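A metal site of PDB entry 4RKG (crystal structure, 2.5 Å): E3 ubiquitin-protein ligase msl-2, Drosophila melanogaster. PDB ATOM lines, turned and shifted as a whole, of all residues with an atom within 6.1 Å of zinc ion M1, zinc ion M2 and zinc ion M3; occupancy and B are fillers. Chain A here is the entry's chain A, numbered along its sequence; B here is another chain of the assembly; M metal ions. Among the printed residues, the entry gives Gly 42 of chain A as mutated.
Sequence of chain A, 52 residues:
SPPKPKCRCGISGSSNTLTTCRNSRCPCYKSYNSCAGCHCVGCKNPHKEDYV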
ATOM      1  N   LYS A   6      20.263 -16.194  13.375  1.00  0.00           N
ATOM      2  CA  LYS A   6      18.955 -16.592  12.797  1.00  0.00           C
ATOM      3  C   LYS A   6      18.014 -15.393  12.541  1.00  0.00           C
ATOM      4  O   LYS A   6      17.309 -14.967  13.455  1.00  0.00           O
ATOM      5  CB  LYS A   6      18.244 -17.585  13.733  1.00  0.00           C
ATOM      6  CG  LYS A   6      18.378 -19.064  13.353  1.00  0.00           C
ATOM      7  CD  LYS A   6      17.868 -19.975  14.472  1.00  0.00           C
ATOM      8  CE  LYS A   6      18.993 -20.353  15.441  1.00  0.00           C
ATOM      9  NZ  LYS A   6      20.094 -21.107  14.766  1.00  0.00           N
ATOM     10  N   CYS A   7      17.981 -14.881  11.302  1.00  0.00           N
ATOM     11  CA  CYS A   7      17.271 -13.624  10.987  1.00  0.00           C
ATOM     12  C   CYS A   7      15.756 -13.782  10.810  1.00  0.00           C
ATOM     13  O   CYS A   7      15.197 -14.886  10.942  1.00  0.00           O
ATOM     14  CB  CYS A   7      17.866 -12.932   9.742  1.00  0.00           C
ATOM     15  SG  CYS A   7      17.802 -13.750   8.121  1.00  0.00           S
ATOM     16  N   ARG A   8      15.095 -12.660  10.555  1.00  0.00           N
ATOM     17  CA  ARG A   8      13.662 -12.630  10.359  1.00  0.00           C
ATOM     18  C   ARG A   8      13.281 -11.529   9.354  1.00  0.00           C
ATOM     19  O   ARG A   8      12.261 -10.841   9.520  1.00  0.00           O
ATOM     20  CB  ARG A   8      12.948 -12.442  11.712  1.00  0.00           C
ATOM     21  CG  ARG A   8      12.582 -13.765  12.373  1.00  0.00           C
ATOM     22  CD  ARG A   8      12.051 -13.562  13.802  1.00  0.00           C
ATOM     23  NE  ARG A   8      10.845 -12.748  13.838  1.00  0.00           N
ATOM     24  CZ  ARG A   8      10.660 -11.703  14.643  1.00  0.00           C
ATOM     25  NH1 ARG A   8       9.525 -11.009  14.586  1.00  0.00           N
ATOM     26  NH2 ARG A   8      11.614 -11.349  15.491  1.00  0.00           N
ATOM     27  N   CYS A   9      14.108 -11.377   8.323  1.00  0.00           N
ATOM     28  CA  CYS A   9      13.861 -10.456   7.209  1.00  0.00           C
ATOM     29  C   CYS A   9      12.725 -10.950   6.314  1.00  0.00           C
ATOM     30  O   CYS A   9      12.705 -12.103   5.941  1.00  0.00           O
ATOM     31  CB  CYS A   9      15.121 -10.278   6.351  1.00  0.00           C
ATOM     32  SG  CYS A   9      16.694 -10.140   7.250  1.00  0.00           S
ATOM     33  N   THR A  20      16.242  -8.536   0.147  1.00  0.00           N
ATOM     34  CA  THR A  20      15.969  -9.257   1.389  1.00  0.00           C
ATOM     35  C   THR A  20      17.066 -10.259   1.706  1.00  0.00           C
ATOM     36  O   THR A  20      17.362 -11.164   0.917  1.00  0.00           O
ATOM     37  CB  THR A  20      14.638 -10.028   1.342  1.00  0.00           C
ATOM     38  OG1 THR A  20      13.547  -9.105   1.421  1.00  0.00           O
ATOM     39  CG2 THR A  20      14.553 -10.982   2.512  1.00  0.00           C
ATOM     40  N   CYS A  21      17.694 -10.073   2.868  1.00  0.00           N
ATOM     41  CA  CYS A  21      18.874 -10.828   3.282  1.00  0.00           C
ATOM     42  C   CYS A  21      20.008 -10.635   2.279  1.00  0.00           C
ATOM     43  O   CYS A  21      20.917 -11.459   2.184  1.00  0.00           O
ATOM     44  CB  CYS A  21      18.563 -12.320   3.435  1.00  0.00           C
ATOM     45  SG  CYS A  21      17.296 -12.724   4.653  1.00  0.00           S
ATOM     46  N   ARG A  22      19.954  -9.546   1.524  1.00  0.00           N
ATOM     47  CA  ARG A  22      21.049  -9.215   0.620  1.00  0.00           C
ATOM     48  C   ARG A  22      21.583  -7.826   0.969  1.00  0.00           C
ATOM     49  O   ARG A  22      21.932  -7.067   0.082  1.00  0.00           O
ATOM     50  CB  ARG A  22      20.605  -9.273  -0.840  1.00  0.00           C
ATOM     51  CG  ARG A  22      21.755  -9.430  -1.818  1.00  0.00           C
ATOM     52  CD  ARG A  22      21.356  -9.125  -3.230  1.00  0.00           C
ATOM     53  NE  ARG A  22      22.395  -9.566  -4.155  1.00  0.00           N
ATOM     54  CZ  ARG A  22      22.473 -10.790  -4.642  1.00  0.00           C
ATOM     55  NH1 ARG A  22      21.571 -11.704  -4.311  1.00  0.00           N
ATOM     56  NH2 ARG A  22      23.454 -11.111  -5.480  1.00  0.00           N
ATOM     57  N   CYS A  26      20.572  -7.152   7.350  1.00  0.00           N
ATOM     58  CA  CYS A  26      20.471  -8.569   7.685  1.00  0.00           C
ATOM     59  C   CYS A  26      21.780  -9.040   8.311  1.00  0.00           C
ATOM     60  O   CYS A  26      22.837  -8.812   7.737  1.00  0.00           O
ATOM     61  CB  CYS A  26      20.125  -9.408   6.435  1.00  0.00           C
ATOM     62  SG  CYS A  26      20.324 -11.220   6.592  1.00  0.00           S
ATOM     63  N   PRO A  27      21.705  -9.665   9.485  1.00  0.00           N
ATOM     64  CA  PRO A  27      22.858 -10.179  10.239  1.00  0.00           C
ATOM     65  C   PRO A  27      23.717 -11.165   9.485  1.00  0.00           C
ATOM     66  O   PRO A  27      24.915 -10.939   9.319  1.00  0.00           O
ATOM     67  CB  PRO A  27      22.214 -10.876  11.448  1.00  0.00           C
ATOM     68  CG  PRO A  27      20.747 -10.877  11.195  1.00  0.00           C
ATOM     69  CD  PRO A  27      20.479  -9.736  10.283  1.00  0.00           C
ATOM     70  N   CYS A  28      23.102 -12.254   9.047  1.00  0.00           N
ATOM     71  CA  CYS A  28      23.799 -13.323   8.335  1.00  0.00           C
ATOM     72  C   CYS A  28      24.567 -12.802   7.116  1.00  0.00           C
ATOM     73  O   CYS A  28      25.734 -13.153   6.917  1.00  0.00           O
ATOM     74  CB  CYS A  28      22.781 -14.383   7.907  1.00  0.00           C
ATOM     75  SG  CYS A  28      21.250 -14.355   8.893  1.00  0.00           S
ATOM     76  N   TYR A  29      23.911 -11.964   6.322  1.00  0.00           N
ATOM     77  CA  TYR A  29      24.561 -11.289   5.214  1.00  0.00           C
ATOM     78  C   TYR A  29      25.792 -10.544   5.722  1.00  0.00           C
ATOM     79  O   TYR A  29      26.909 -10.815   5.303  1.00  0.00           O
ATOM     80  CB  TYR A  29      23.606 -10.304   4.527  1.00  0.00           C
ATOM     81  CG  TYR A  29      23.975  -9.934   3.111  1.00  0.00           C
ATOM     82  CD1 TYR A  29      23.840 -10.852   2.069  1.00  0.00           C
ATOM     83  CD2 TYR A  29      24.449  -8.673   2.797  1.00  0.00           C
ATOM     84  CE1 TYR A  29      24.160 -10.523   0.766  1.00  0.00           C
ATOM     85  CE2 TYR A  29      24.781  -8.330   1.486  1.00  0.00           C
ATOM     86  CZ  TYR A  29      24.627  -9.259   0.475  1.00  0.00           C
ATOM     87  OH  TYR A  29      24.947  -8.930  -0.828  1.00  0.00           O
ATOM     88  N   ASN A  33      27.410 -14.920   6.543  1.00  0.00           N
ATOM     89  CA  ASN A  33      26.904 -16.281   6.665  1.00  0.00           C
ATOM     90  C   ASN A  33      25.590 -16.451   5.925  1.00  0.00           C
ATOM     91  O   ASN A  33      24.944 -15.465   5.568  1.00  0.00           O
ATOM     92  CB  ASN A  33      26.720 -16.661   8.140  1.00  0.00           C
ATOM     93  CG  ASN A  33      27.961 -16.415   8.940  1.00  0.00           C
ATOM     94  OD1 ASN A  33      28.069 -15.404   9.633  1.00  0.00           O
ATOM     95  ND2 ASN A  33      28.931 -17.335   8.837  1.00  0.00           N
ATOM     96  N   SER A  34      25.205 -17.701   5.676  1.00  0.00           N
ATOM     97  CA  SER A  34      23.968 -18.015   4.968  1.00  0.00           C
ATOM     98  C   SER A  34      22.759 -17.934   5.897  1.00  0.00           C
ATOM     99  O   SER A  34      22.904 -17.631   7.084  1.00  0.00           O
ATOM    100  CB  SER A  34      24.046 -19.418   4.351  1.00  0.00           C
ATOM    101  OG  SER A  34      24.099 -20.408   5.375  1.00  0.00           O
ATOM    102  N   CYS A  35      21.577 -18.197   5.373  1.00  0.00           N
ATOM    103  CA  CYS A  35      20.376 -18.185   6.208  1.00  0.00           C
ATOM    104  C   CYS A  35      19.940 -19.600   6.526  1.00  0.00           C
ATOM    105  O   CYS A  35      18.756 -19.931   6.485  1.00  0.00           O
ATOM    106  CB  CYS A  35      19.257 -17.403   5.540  1.00  0.00           C
ATOM    107  SG  CYS A  35      19.532 -15.658   5.576  1.00  0.00           S
ATOM    108  N   ALA A  36      20.912 -20.452   6.827  1.00  0.00           N
ATOM    109  CA  ALA A  36      20.639 -21.795   7.299  1.00  0.00           C
ATOM    110  C   ALA A  36      19.892 -21.731   8.629  1.00  0.00           C
ATOM    111  O   ALA A  36      20.444 -21.261   9.628  1.00  0.00           O
ATOM    112  CB  ALA A  36      21.949 -22.576   7.438  1.00  0.00           C
ATOM    113  N   CYS A  38      17.318 -19.907   9.357  1.00  0.00           N
ATOM    114  CA  CYS A  38      16.661 -18.614   9.545  1.00  0.00           C
ATOM    115  C   CYS A  38      15.138 -18.673   9.358  1.00  0.00           C
ATOM    116  O   CYS A  38      14.600 -19.674   8.916  1.00  0.00           O
ATOM    117  CB  CYS A  38      17.243 -17.568   8.587  1.00  0.00           C
ATOM    118  SG  CYS A  38      18.877 -16.854   9.000  1.00  0.00           S
ATOM    119  N   HIS A  39      14.462 -17.588   9.680  1.00  0.00           N
ATOM    120  CA  HIS A  39      13.003 -17.538   9.564  1.00  0.00           C
ATOM    121  C   HIS A  39      12.544 -16.453   8.589  1.00  0.00           C
ATOM    122  O   HIS A  39      11.366 -16.123   8.516  1.00  0.00           O
ATOM    123  CB  HIS A  39      12.409 -17.341  10.961  1.00  0.00           C
ATOM    124  CG  HIS A  39      12.460 -18.578  11.775  1.00  0.00           C
ATOM    125  ND1 HIS A  39      12.642 -18.575  13.142  1.00  0.00           N
ATOM    126  CD2 HIS A  39      12.397 -19.887  11.410  1.00  0.00           C
ATOM    127  CE1 HIS A  39      12.661 -19.827  13.581  1.00  0.00           C
ATOM    128  NE2 HIS A  39      12.516 -20.635  12.548  1.00  0.00           N
ATOM    129  N   CYS A  40      13.502 -15.920   7.855  1.00  0.00           N
ATOM    130  CA  CYS A  40      13.280 -15.004   6.744  1.00  0.00           C
ATOM    131  C   CYS A  40      12.280 -15.520   5.701  1.00  0.00           C
ATOM    132  O   CYS A  40      11.969 -16.710   5.629  1.00  0.00           O
ATOM    133  CB  CYS A  40      14.623 -14.697   6.076  1.00  0.00           C
ATOM    134  SG  CYS A  40      15.686 -16.174   5.827  1.00  0.00           S
ATOM    135  N   VAL A  41      11.777 -14.612   4.881  1.00  0.00           N
ATOM    136  CA  VAL A  41      10.795 -14.927   3.848  1.00  0.00           C
ATOM    137  C   VAL A  41      11.252 -14.235   2.574  1.00  0.00           C
ATOM    138  O   VAL A  41      11.640 -13.074   2.605  1.00  0.00           O
ATOM    139  CB  VAL A  41       9.376 -14.449   4.243  1.00  0.00           C
ATOM    140  CG1 VAL A  41       8.374 -14.769   3.196  1.00  0.00           C
ATOM    141  CG2 VAL A  41       8.947 -15.058   5.586  1.00  0.00           C
ATOM    142  N   GLY A  42      11.234 -14.951   1.465  1.00  0.00           N
ATOM    143  CA  GLY A  42      11.705 -14.383   0.215  1.00  0.00           C
ATOM    144  C   GLY A  42      13.173 -14.018   0.368  1.00  0.00           C
ATOM    145  O   GLY A  42      13.601 -12.945  -0.058  1.00  0.00           O
ATOM    146  N   CYS A  43      13.917 -14.916   0.996  1.00  0.00           N
ATOM    147  CA  CYS A  43      15.358 -14.752   1.175  1.00  0.00           C
ATOM    148  C   CYS A  43      16.067 -14.661  -0.158  1.00  0.00           C
ATOM    149  O   CYS A  43      15.777 -15.424  -1.066  1.00  0.00           O
ATOM    150  CB  CYS A  43      15.936 -15.907   1.986  1.00  0.00           C
ATOM    151  SG  CYS A  43      17.708 -15.641   2.375  1.00  0.00           S
ATOM    152  N   LYS A  44      16.998 -13.729  -0.276  1.00  0.00           N
ATOM    153  CA  LYS A  44      17.776 -13.592  -1.492  1.00  0.00           C
ATOM    154  C   LYS A  44      19.237 -13.541  -1.097  1.00  0.00           C
ATOM    155  O   LYS A  44      20.077 -13.036  -1.828  1.00  0.00           O
ATOM    156  CB  LYS A  44      17.362 -12.346  -2.272  1.00  0.00           C
ATOM    157  CG  LYS A  44      15.869 -12.234  -2.565  1.00  0.00           C
ATOM    158  CD  LYS A  44      15.566 -12.499  -4.012  1.00  0.00           C
ATOM    159  CE  LYS A  44      14.456 -11.600  -4.571  1.00  0.00           C
ATOM    160  NZ  LYS A  44      13.226 -11.572  -3.752  1.00  0.00           N
ATOM    161  N   ASN A  45      19.532 -14.066   0.078  1.00  0.00           N
ATOM    162  CA  ASN A  45      20.899 -14.249   0.518  1.00  0.00           C
ATOM    163  C   ASN A  45      21.636 -15.197  -0.410  1.00  0.00           C
ATOM    164  O   ASN A  45      21.300 -16.373  -0.466  1.00  0.00           O
ATOM    165  CB  ASN A  45      20.928 -14.790   1.938  1.00  0.00           C
ATOM    166  CG  ASN A  45      22.296 -14.710   2.563  1.00  0.00           C
ATOM    167  OD1 ASN A  45      23.309 -14.666   1.864  1.00  0.00           O
ATOM    168  ND2 ASN A  45      22.343 -14.673   3.891  1.00  0.00           N
ATOM    169  P    DG B   5      14.012  -6.527   6.983  1.00  0.00           P
ATOM    170  OP1  DG B   5      14.935  -6.537   5.819  1.00  0.00           O
ATOM    171  OP2  DG B   5      12.678  -7.160   6.904  1.00  0.00           O
ATOM    172  O5'  DG B   5      14.790  -7.126   8.242  1.00  0.00           O
ATOM    173  C5'  DG B   5      16.060  -6.612   8.555  1.00  0.00           C
ATOM    174  C4'  DG B   5      16.368  -6.740  10.031  1.00  0.00           C
ATOM    175  O4'  DG B   5      15.614  -5.757  10.783  1.00  0.00           O
ATOM    176  C3'  DG B   5      16.010  -8.066  10.669  1.00  0.00           C
ATOM    177  O3'  DG B   5      16.891  -8.249  11.737  1.00  0.00           O
ATOM    178  C2'  DG B   5      14.577  -7.826  11.147  1.00  0.00           C
ATOM    179  C1'  DG B   5      14.684  -6.394  11.630  1.00  0.00           C
ATOM    180  N9   DG B   5      13.453  -5.660  11.498  1.00  0.00           N
ATOM    181  C8   DG B   5      12.594  -5.665  10.424  1.00  0.00           C
ATOM    182  N7   DG B   5      11.589  -4.850  10.565  1.00  0.00           N
ATOM    183  C5   DG B   5      11.823  -4.239  11.789  1.00  0.00           C
ATOM    184  C6   DG B   5      11.069  -3.262  12.477  1.00  0.00           C
ATOM    185  O6   DG B   5      10.011  -2.724  12.107  1.00  0.00           O
ATOM    186  N1   DG B   5      11.649  -2.925  13.694  1.00  0.00           N
ATOM    187  C2   DG B   5      12.803  -3.478  14.186  1.00  0.00           C
ATOM    188  N2   DG B   5      13.203  -3.026  15.393  1.00  0.00           N
ATOM    189  N3   DG B   5      13.516  -4.389  13.561  1.00  0.00           N
ATOM    190  C4   DG B   5      12.966  -4.725  12.366  1.00  0.00           C
ATOM    191  P    DC B   6      16.791  -9.548  12.649  1.00  0.00           P
ATOM    192  OP1  DC B   6      18.197  -9.843  13.016  1.00  0.00           O
ATOM    193  OP2  DC B   6      15.940 -10.573  12.016  1.00  0.00           O
ATOM    194  O5'  DC B   6      16.041  -9.013  13.942  1.00  0.00           O
ATOM    195  C5'  DC B   6      16.619  -7.979  14.698  1.00  0.00           C
ATOM    196  C4'  DC B   6      15.753  -7.667  15.888  1.00  0.00           C
ATOM    197  O4'  DC B   6      14.546  -6.998  15.429  1.00  0.00           O
ATOM    198  C3'  DC B   6      15.281  -8.886  16.690  1.00  0.00           C
ATOM    199  O3'  DC B   6      15.181  -8.519  18.042  1.00  0.00           O
ATOM    200  C2'  DC B   6      13.893  -9.130  16.091  1.00  0.00           C
ATOM    201  C1'  DC B   6      13.434  -7.691  15.961  1.00  0.00           C
ATOM    202  N1   DC B   6      12.268  -7.476  15.067  1.00  0.00           N
ATOM    203  C2   DC B   6      11.365  -6.463  15.374  1.00  0.00           C
ATOM    204  O2   DC B   6      11.570  -5.778  16.373  1.00  0.00           O
ATOM    205  N3   DC B   6      10.312  -6.239  14.570  1.00  0.00           N
ATOM    206  C4   DC B   6      10.146  -7.003  13.480  1.00  0.00           C
ATOM    207  N4   DC B   6       9.080  -6.753  12.706  1.00  0.00           N
ATOM    208  C5   DC B   6      11.050  -8.057  13.150  1.00  0.00           C
ATOM    209  C6   DC B   6      12.097  -8.259  13.961  1.00  0.00           C
HETATM  210 ZN    ZN M   1      19.316 -15.123   7.738  1.00  0.00          ZN
HETATM  211 ZN    ZN M   2      18.107 -11.958   6.738  1.00  0.00          ZN
HETATM  212 ZN    ZN M   3      17.496 -14.932   4.505  1.00  0.00          ZN
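The backbone carbonyl oxygen (O) of Cys 28 sits at hydrogen-bond distance from the backbone NH (N) of Asn 33 (2.5 Å). The backbone NH (N) of Tyr 29 lies close to the side-chain sulfur (SG) of Cys 26 (3.7 Å). The side-chain sulfur (SG) of Cys 43 lies close to the backbone NH (N) of Asn 45, 3.3 Å away. O5' of DG 5 of chain B lies close to SG of Cys 9 (3.7 Å). The backbone carbonyl oxygen (O) of Cys 9 is in hydrogen-bond range of the backbone NH (N) of Val 41, at 2.9 Å. The backbone NH (N) of His 39 is in hydrogen-bond range of the backbone carbonyl oxygen (O) of Cys 7 (3.1 Å). ND2 of Asn 45 sits close to SG of Cys 35.
Within 4 Å of zinc ion M1: Cys 7, Cys 28, Cys 35 and Cys 38.
Four residues have an atom within 4 Å of zinc ion M2: Cys 7, Cys 9, Cys 21 and Cys 26. The nearest printed residue that does not touch zinc ion M2 is Cys 35 (4.1 Å).
Five residues have an atom within 4 Å of zinc ion M3: Cys 7, Cys 21, Cys 35, Cys 40 and Cys 43. The nearest printed residue that does not touch zinc ion M3 is Asn 45 (4.3 Å).
Zinc ion M1 is bound by the side-chain sulfur of Cys 7 (2.1 Å), the side-chain sulfur of Cys 38 (2.2 Å), the side-chain sulfur of Cys 35 (2.2 Å) and the side-chain sulfur of Cys 28 (2.4 Å). Zinc ion M1 has four donor atoms within binding distance.
Zinc ion M2 is bound by the side-chain sulfur of Cys 7, the side-chain sulfur of Cys 26, the side-chain sulfur of Cys 9 and the side-chain sulfur of Cys 21. Zinc ion M2 has four donor atoms within binding distance.
Zinc ion M3 is bound by the side-chain sulfur (SG) of Cys 21 (2.2 Å), the side-chain sulfur (SG) of Cys 43 (2.3 Å), the side-chain sulfur (SG) of Cys 35 (2.4 Å) and the side-chain sulfur (SG) of Cys 40 (2.6 Å). Zinc ion M3 has four donor atoms within binding distance.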
